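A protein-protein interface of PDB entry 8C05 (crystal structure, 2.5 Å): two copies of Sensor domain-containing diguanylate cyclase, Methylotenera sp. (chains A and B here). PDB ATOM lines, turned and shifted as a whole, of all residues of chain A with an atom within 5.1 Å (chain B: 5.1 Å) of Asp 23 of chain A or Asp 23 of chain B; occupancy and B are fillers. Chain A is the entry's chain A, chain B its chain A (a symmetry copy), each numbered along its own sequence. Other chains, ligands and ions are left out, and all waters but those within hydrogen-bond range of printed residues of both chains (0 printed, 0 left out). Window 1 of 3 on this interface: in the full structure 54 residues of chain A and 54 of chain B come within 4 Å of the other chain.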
ATOM      1  N   ALA A  21      -3.713  22.054 -30.647  1.00  0.00           N
ATOM      2  CA  ALA A  21      -4.600  21.104 -29.994  1.00  0.00           C
ATOM      3  C   ALA A  21      -5.317  20.257 -31.043  1.00  0.00           C
ATOM      4  O   ALA A  21      -5.011  20.315 -32.239  1.00  0.00           O
ATOM      5  CB  ALA A  21      -5.590  21.845 -29.091  1.00  0.00           C
ATOM      6  N   ARG A  22      -6.279  19.455 -30.587  1.00  0.00           N
ATOM      7  CA  ARG A  22      -7.116  18.664 -31.477  1.00  0.00           C
ATOM      8  C   ARG A  22      -8.532  19.211 -31.592  1.00  0.00           C
ATOM      9  O   ARG A  22      -9.326  18.681 -32.377  1.00  0.00           O
ATOM     10  CB  ARG A  22      -7.153  17.201 -31.016  1.00  0.00           C
ATOM     11  CG  ARG A  22      -5.811  16.490 -31.128  1.00  0.00           C
ATOM     12  CD  ARG A  22      -5.116  16.405 -29.782  1.00  0.00           C
ATOM     13  NE  ARG A  22      -5.646  15.314 -28.973  1.00  0.00           N
ATOM     14  CZ  ARG A  22      -5.410  15.157 -27.678  1.00  0.00           C
ATOM     15  NH1 ARG A  22      -4.675  16.022 -27.000  1.00  0.00           N
ATOM     16  NH2 ARG A  22      -5.928  14.107 -27.047  1.00  0.00           N
ATOM     17  N   ASP A  23      -8.868  20.248 -30.833  1.00  0.00           N
ATOM     18  CA  ASP A  23     -10.115  20.981 -30.995  1.00  0.00           C
ATOM     19  C   ASP A  23      -9.817  22.327 -31.641  1.00  0.00           C
ATOM     20  O   ASP A  23      -8.796  22.955 -31.343  1.00  0.00           O
ATOM     21  CB  ASP A  23     -10.823  21.186 -29.652  1.00  0.00           C
ATOM     22  CG  ASP A  23     -11.438  19.907 -29.116  1.00  0.00           C
ATOM     23  OD1 ASP A  23     -11.389  18.878 -29.822  1.00  0.00           O
ATOM     24  OD2 ASP A  23     -11.973  19.931 -27.987  1.00  0.00           O
ATOM     25  N   GLY A  24     -10.705  22.761 -32.530  1.00  0.00           N
ATOM     26  CA  GLY A  24     -10.484  24.013 -33.231  1.00  0.00           C
ATOM     27  C   GLY A  24     -10.503  25.196 -32.279  1.00  0.00           C
ATOM     28  O   GLY A  24     -11.313  25.267 -31.355  1.00  0.00           O
ATOM     29  N   ILE A  25      -9.587  26.134 -32.508  1.00  0.00           N
ATOM     30  CA  ILE A  25      -9.487  27.355 -31.717  1.00  0.00           C
ATOM     31  C   ILE A  25      -9.561  28.537 -32.672  1.00  0.00           C
ATOM     32  O   ILE A  25      -8.715  28.677 -33.564  1.00  0.00           O
ATOM     33  CB  ILE A  25      -8.193  27.401 -30.890  1.00  0.00           C
ATOM     34  CG1 ILE A  25      -8.189  26.283 -29.845  1.00  0.00           C
ATOM     35  CG2 ILE A  25      -8.037  28.761 -30.224  1.00  0.00           C
ATOM     36  CD1 ILE A  25      -6.980  26.301 -28.935  1.00  0.00           C
ATOM     37  N   ASN A  41      -6.388  28.290 -35.610  1.00  0.00           N
ATOM     38  CA  ASN A  41      -5.317  27.371 -35.263  1.00  0.00           C
ATOM     39  C   ASN A  41      -5.248  26.232 -36.282  1.00  0.00           C
ATOM     40  O   ASN A  41      -6.027  26.164 -37.235  1.00  0.00           O
ATOM     41  CB  ASN A  41      -5.508  26.832 -33.844  1.00  0.00           C
ATOM     42  CG  ASN A  41      -6.668  25.858 -33.736  1.00  0.00           C
ATOM     43  OD1 ASN A  41      -7.644  25.946 -34.483  1.00  0.00           O
ATOM     44  ND2 ASN A  41      -6.569  24.925 -32.796  1.00  0.00           N
ATOM     45  N   ALA A  43      -5.801  22.999 -35.697  1.00  0.00           N
ATOM     46  CA  ALA A  43      -6.873  22.025 -35.521  1.00  0.00           C
ATOM     47  C   ALA A  43      -8.134  22.429 -36.272  1.00  0.00           C
ATOM     48  O   ALA A  43      -8.894  21.561 -36.715  1.00  0.00           O
ATOM     49  CB  ALA A  43      -7.178  21.840 -34.036  1.00  0.00           C
ATOM     50  N   MET A  47      -9.929  20.152 -39.059  1.00  0.00           N
ATOM     51  CA  MET A  47     -11.283  19.675 -38.811  1.00  0.00           C
ATOM     52  C   MET A  47     -12.253  20.112 -39.899  1.00  0.00           C
ATOM     53  O   MET A  47     -13.179  19.363 -40.233  1.00  0.00           O
ATOM     54  CB  MET A  47     -11.770  20.170 -37.449  1.00  0.00           C
ATOM     55  CG  MET A  47     -13.094  19.572 -37.005  1.00  0.00           C
ATOM     56  SD  MET A  47     -13.702  20.352 -35.500  1.00  0.00           S
ATOM     57  CE  MET A  47     -12.292  20.128 -34.420  1.00  0.00           C
ATOM     58  N   ILE A 122     -14.351  27.535 -29.611  1.00  0.00           N
ATOM     59  CA  ILE A 122     -13.707  26.232 -29.497  1.00  0.00           C
ATOM     60  C   ILE A 122     -14.621  25.206 -30.154  1.00  0.00           C
ATOM     61  O   ILE A 122     -15.732  24.951 -29.672  1.00  0.00           O
ATOM     62  CB  ILE A 122     -13.415  25.865 -28.037  1.00  0.00           C
ATOM     63  CG1 ILE A 122     -12.617  26.980 -27.361  1.00  0.00           C
ATOM     64  CG2 ILE A 122     -12.644  24.557 -27.967  1.00  0.00           C
ATOM     65  CD1 ILE A 122     -11.238  27.176 -27.947  1.00  0.00           C
ATOM     66  N   GLN A 123     -14.155  24.615 -31.250  1.00  0.00           N
ATOM     67  CA  GLN A 123     -14.908  23.607 -31.984  1.00  0.00           C
ATOM     68  C   GLN A 123     -14.396  22.219 -31.619  1.00  0.00           C
ATOM     69  O   GLN A 123     -13.194  21.950 -31.718  1.00  0.00           O
ATOM     70  CB  GLN A 123     -14.795  23.826 -33.494  1.00  0.00           C
ATOM     71  CG  GLN A 123     -15.347  25.157 -33.987  1.00  0.00           C
ATOM     72  CD  GLN A 123     -14.374  26.306 -33.802  1.00  0.00           C
ATOM     73  OE1 GLN A 123     -13.232  26.109 -33.387  1.00  0.00           O
ATOM     74  NE2 GLN A 123     -14.823  27.517 -34.112  1.00  0.00           N
ATOM     75  N   LYS A 124     -15.308  21.344 -31.202  1.00  0.00           N
ATOM     76  CA  LYS A 124     -14.978  19.979 -30.809  1.00  0.00           C
ATOM     77  C   LYS A 124     -15.793  19.012 -31.655  1.00  0.00           C
ATOM     78  O   LYS A 124     -17.027  19.045 -31.623  1.00  0.00           O
ATOM     79  CB  LYS A 124     -15.252  19.754 -29.321  1.00  0.00           C
ATOM     80  CG  LYS A 124     -15.048  18.321 -28.856  1.00  0.00           C
ATOM     81  CD  LYS A 124     -15.438  18.161 -27.395  1.00  0.00           C
ATOM     82  CE  LYS A 124     -15.320  16.714 -26.941  1.00  0.00           C
ATOM     83  NZ  LYS A 124     -13.916  16.223 -26.990  1.00  0.00           N
ATOM     84  N   ASP A 125     -15.104  18.157 -32.409  1.00  0.00           N
ATOM     85  CA  ASP A 125     -15.776  17.174 -33.251  1.00  0.00           C
ATOM     86  C   ASP A 125     -16.431  16.121 -32.364  1.00  0.00           C
ATOM     87  O   ASP A 125     -15.745  15.273 -31.784  1.00  0.00           O
ATOM     88  CB  ASP A 125     -14.782  16.538 -34.219  1.00  0.00           C
ATOM     89  CG  ASP A 125     -15.464  15.793 -35.355  1.00  0.00           C
ATOM     90  OD1 ASP A 125     -16.563  15.238 -35.140  1.00  0.00           O
ATOM     91  OD2 ASP A 125     -14.903  15.767 -36.469  1.00  0.00           O
ATOM     92  N   ALA B  21     -11.629  24.472 -20.703  1.00  0.00           N
ATOM     93  CA  ALA B  21     -11.959  23.740 -21.916  1.00  0.00           C
ATOM     94  C   ALA B  21     -12.760  22.488 -21.565  1.00  0.00           C
ATOM     95  O   ALA B  21     -13.171  22.285 -20.417  1.00  0.00           O
ATOM     96  CB  ALA B  21     -10.681  23.397 -22.685  1.00  0.00           C
ATOM     97  N   ARG B  22     -12.990  21.643 -22.569  1.00  0.00           N
ATOM     98  CA  ARG B  22     -13.653  20.362 -22.369  1.00  0.00           C
ATOM     99  C   ARG B  22     -12.694  19.184 -22.464  1.00  0.00           C
ATOM    100  O   ARG B  22     -13.109  18.043 -22.235  1.00  0.00           O
ATOM    101  CB  ARG B  22     -14.799  20.190 -23.374  1.00  0.00           C
ATOM    102  CG  ARG B  22     -15.944  21.174 -23.171  1.00  0.00           C
ATOM    103  CD  ARG B  22     -15.872  22.319 -24.165  1.00  0.00           C
ATOM    104  NE  ARG B  22     -16.410  21.935 -25.465  1.00  0.00           N
ATOM    105  CZ  ARG B  22     -16.252  22.636 -26.578  1.00  0.00           C
ATOM    106  NH1 ARG B  22     -15.550  23.756 -26.595  1.00  0.00           N
ATOM    107  NH2 ARG B  22     -16.808  22.199 -27.704  1.00  0.00           N
ATOM    108  N   ASP B  23     -11.431  19.428 -22.797  1.00  0.00           N
ATOM    109  CA  ASP B  23     -10.382  18.422 -22.726  1.00  0.00           C
ATOM    110  C   ASP B  23      -9.487  18.723 -21.532  1.00  0.00           C
ATOM    111  O   ASP B  23      -9.210  19.889 -21.232  1.00  0.00           O
ATOM    112  CB  ASP B  23      -9.550  18.388 -24.012  1.00  0.00           C
ATOM    113  CG  ASP B  23     -10.303  17.775 -25.178  1.00  0.00           C
ATOM    114  OD1 ASP B  23     -11.440  17.300 -24.971  1.00  0.00           O
ATOM    115  OD2 ASP B  23      -9.757  17.766 -26.301  1.00  0.00           O
ATOM    116  N   GLY B  24      -9.046  17.672 -20.847  1.00  0.00           N
ATOM    117  CA  GLY B  24      -8.223  17.862 -19.667  1.00  0.00           C
ATOM    118  C   GLY B  24      -6.888  18.498 -20.013  1.00  0.00           C
ATOM    119  O   GLY B  24      -6.262  18.172 -21.022  1.00  0.00           O
ATOM    120  N   ILE B  25      -6.455  19.425 -19.163  1.00  0.00           N
ATOM    121  CA  ILE B  25      -5.176  20.109 -19.320  1.00  0.00           C
ATOM    122  C   ILE B  25      -4.384  19.919 -18.036  1.00  0.00           C
ATOM    123  O   ILE B  25      -4.828  20.336 -16.958  1.00  0.00           O
ATOM    124  CB  ILE B  25      -5.356  21.602 -19.635  1.00  0.00           C
ATOM    125  CG1 ILE B  25      -6.040  21.782 -20.993  1.00  0.00           C
ATOM    126  CG2 ILE B  25      -4.012  22.315 -19.611  1.00  0.00           C
ATOM    127  CD1 ILE B  25      -6.190  23.226 -21.415  1.00  0.00           C
ATOM    128  N   ASN B  41      -6.608  21.476 -14.661  1.00  0.00           N
ATOM    129  CA  ASN B  41      -7.705  22.360 -15.020  1.00  0.00           C
ATOM    130  C   ASN B  41      -9.038  21.752 -14.582  1.00  0.00           C
ATOM    131  O   ASN B  41      -9.100  20.659 -14.015  1.00  0.00           O
ATOM    132  CB  ASN B  41      -7.696  22.649 -16.522  1.00  0.00           C
ATOM    133  CG  ASN B  41      -8.109  21.448 -17.354  1.00  0.00           C
ATOM    134  OD1 ASN B  41      -7.901  20.299 -16.960  1.00  0.00           O
ATOM    135  ND2 ASN B  41      -8.694  21.710 -18.517  1.00  0.00           N
ATOM    136  N   ALA B  43     -11.530  20.778 -16.567  1.00  0.00           N
ATOM    137  CA  ALA B  43     -11.956  19.682 -17.432  1.00  0.00           C
ATOM    138  C   ALA B  43     -11.367  18.350 -16.990  1.00  0.00           C
ATOM    139  O   ALA B  43     -11.993  17.302 -17.185  1.00  0.00           O
ATOM    140  CB  ALA B  43     -11.573  19.975 -18.882  1.00  0.00           C
ATOM    141  N   MET B  47     -13.560  15.116 -16.038  1.00  0.00           N
ATOM    142  CA  MET B  47     -13.422  13.911 -16.846  1.00  0.00           C
ATOM    143  C   MET B  47     -13.008  12.707 -16.013  1.00  0.00           C
ATOM    144  O   MET B  47     -13.436  11.584 -16.302  1.00  0.00           O
ATOM    145  CB  MET B  47     -12.408  14.146 -17.965  1.00  0.00           C
ATOM    146  CG  MET B  47     -12.330  13.021 -18.982  1.00  0.00           C
ATOM    147  SD  MET B  47     -10.978  13.270 -20.145  1.00  0.00           S
ATOM    148  CE  MET B  47     -11.364  14.908 -20.754  1.00  0.00           C
ATOM    149  N   ILE B 122      -2.649  16.700 -22.501  1.00  0.00           N
ATOM    150  CA  ILE B 122      -4.000  17.025 -22.940  1.00  0.00           C
ATOM    151  C   ILE B 122      -4.774  15.719 -23.060  1.00  0.00           C
ATOM    152  O   ILE B 122      -4.459  14.874 -23.908  1.00  0.00           O
ATOM    153  CB  ILE B 122      -4.000  17.796 -24.266  1.00  0.00           C
ATOM    154  CG1 ILE B 122      -3.100  19.028 -24.161  1.00  0.00           C
ATOM    155  CG2 ILE B 122      -5.414  18.216 -24.632  1.00  0.00           C
ATOM    156  CD1 ILE B 122      -3.594  20.054 -23.168  1.00  0.00           C
ATOM    157  N   GLN B 123      -5.788  15.553 -22.216  1.00  0.00           N
ATOM    158  CA  GLN B 123      -6.626  14.362 -22.214  1.00  0.00           C
ATOM    159  C   GLN B 123      -7.931  14.654 -22.944  1.00  0.00           C
ATOM    160  O   GLN B 123      -8.631  15.617 -22.614  1.00  0.00           O
ATOM    161  CB  GLN B 123      -6.918  13.896 -20.786  1.00  0.00           C
ATOM    162  CG  GLN B 123      -5.686  13.504 -19.981  1.00  0.00           C
ATOM    163  CD  GLN B 123      -4.963  14.698 -19.386  1.00  0.00           C
ATOM    164  OE1 GLN B 123      -5.426  15.834 -19.488  1.00  0.00           O
ATOM    165  NE2 GLN B 123      -3.821  14.445 -18.756  1.00  0.00           N
ATOM    166  N   LYS B 124      -8.256  13.820 -23.930  1.00  0.00           N
ATOM    167  CA  LYS B 124      -9.467  13.967 -24.728  1.00  0.00           C
ATOM    168  C   LYS B 124     -10.280  12.685 -24.630  1.00  0.00           C
ATOM    169  O   LYS B 124      -9.798  11.612 -25.009  1.00  0.00           O
ATOM    170  CB  LYS B 124      -9.130  14.280 -26.186  1.00  0.00           C
ATOM    171  CG  LYS B 124     -10.334  14.330 -27.112  1.00  0.00           C
ATOM    172  CD  LYS B 124      -9.905  14.543 -28.555  1.00  0.00           C
ATOM    173  CE  LYS B 124     -11.095  14.510 -29.502  1.00  0.00           C
ATOM    174  NZ  LYS B 124     -12.049  15.623 -29.245  1.00  0.00           N
ATOM    175  N   ASP B 125     -11.506  12.796 -24.124  1.00  0.00           N
ATOM    176  CA  ASP B 125     -12.384  11.638 -23.995  1.00  0.00           C
ATOM    177  C   ASP B 125     -12.820  11.184 -25.383  1.00  0.00           C
ATOM    178  O   ASP B 125     -13.646  11.838 -26.028  1.00  0.00           O
ATOM    179  CB  ASP B 125     -13.590  11.982 -23.124  1.00  0.00           C
ATOM    180  CG  ASP B 125     -14.338  10.748 -22.646  1.00  0.00           C
ATOM    181  OD1 ASP B 125     -14.372   9.739 -23.382  1.00  0.00           O
ATOM    182  OD2 ASP B 125     -14.892  10.786 -21.528  1.00  0.00           O
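The side-chain amino group (NZ) of Lys 124 of chain A lies close to the side-chain amino group (NZ) of Lys 124 of chain B (3.0 Å).
The backbone carbonyl oxygen of Ile 122 of chain A sits at hydrogen-bond distance from the guanidinium group of Arg 22 of chain B (3.3 Å).
NZ of Lys 124 of chain A is in salt-bridge range of OD1 of Asp 23 of chain B.
The side-chain amino group (NZ) of Lys 124 of chain B lies within salt-bridge range of the side-chain carboxylate (OD1) of Asp 23 of chain A, at 3.4 Å.
The guanidinium group (NH1) of Arg 22 of chain A sits at hydrogen-bond distance from the backbone carbonyl oxygen (O) of Ile 122 of chain B, at 3.3 Å.
The side-chain amide nitrogen of Asn 41 of chain A lies within hydrogen-bond range of the backbone carbonyl oxygen of Asp 23 of chain A (3.3 Å).
The side-chain amide nitrogen of Asn 41 of chain B is in hydrogen-bond range of the backbone carbonyl oxygen of Asp 23 of chain B (3.3 Å).
NH2 of Arg 22 of chain A touches CB of Lys 124 of chain B, at 3.3 Å.
Asp 23 of chain A touches Asp 23 of chain B.
Arg 22 of chain B touches Lys 124 of chain A.
Of chain B, only Asp 23 (3.5 Å) and Lys 124 (3.4 Å) come within 4 Å of Asp 23 of chain A.
Asp 23 of chain B touches two residues of chain A.
Of the printed residues of chain B, Lys 124 of chain A touches Arg 22, Asp 23 and Lys 124.
Printed residues of chain A within 4 Å of Ile 122 of chain B: Arg 22 (3.3 Å).
Of the printed residues of chain B, Arg 22 of chain A touches Ile 122 and Lys 124.
Printed residues of chain B within 4 Å of Ile 122 of chain A: Arg 22 (3.3 Å).
Ile 25 of chain B touches none of the printed residues of chain A.
The nearest printed residue of chain A that does not touch Asp 23 of chain B is Arg 22 of chain A (5.3 Å).
The nearest printed residue of chain A that does not touch Arg 22 of chain B is Gln 123 of chain A (4.6 Å).
Of the 12 printed residues of chain A, 4 touch a printed residue of chain B.
Printed residues of chain A that touch a printed residue of chain B: Arg 22, Asp 23, Ile 122 and Lys 124.
Of the 12 printed residues of chain B, 4 touch a printed residue of chain A.
Among the printed residues, 8 pairs touch across the chains.
Among the printed residues, Asp or Glu carboxylates within 4 Å of a Lys or Arg side-chain nitrogen of the other chain: Asp 23 of chain A with Lys 124 of chain B (3.4 Å) and Lys 124 of chain A with Asp 23 of chain B (3.4 Å).
Arg 22 of chain A touches Lys 124 of chain B, and with the chains exchanged Lys 124 of chain A touches Arg 22 of chain B.
Asp 23 of chain A touches its own counterpart, Asp 23 of chain B.
Asp 23 of chain A touches Lys 124 of chain B, and with the chains exchanged Lys 124 of chain A touches Asp 23 of chain B.
Lys 124 of chain B touches its own counterpart, Lys 124 of chain A.
Positions printed for both chains: 21, 22, 23, 24, 25, 41, 43, 47, 122, 123, 124 and 125.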
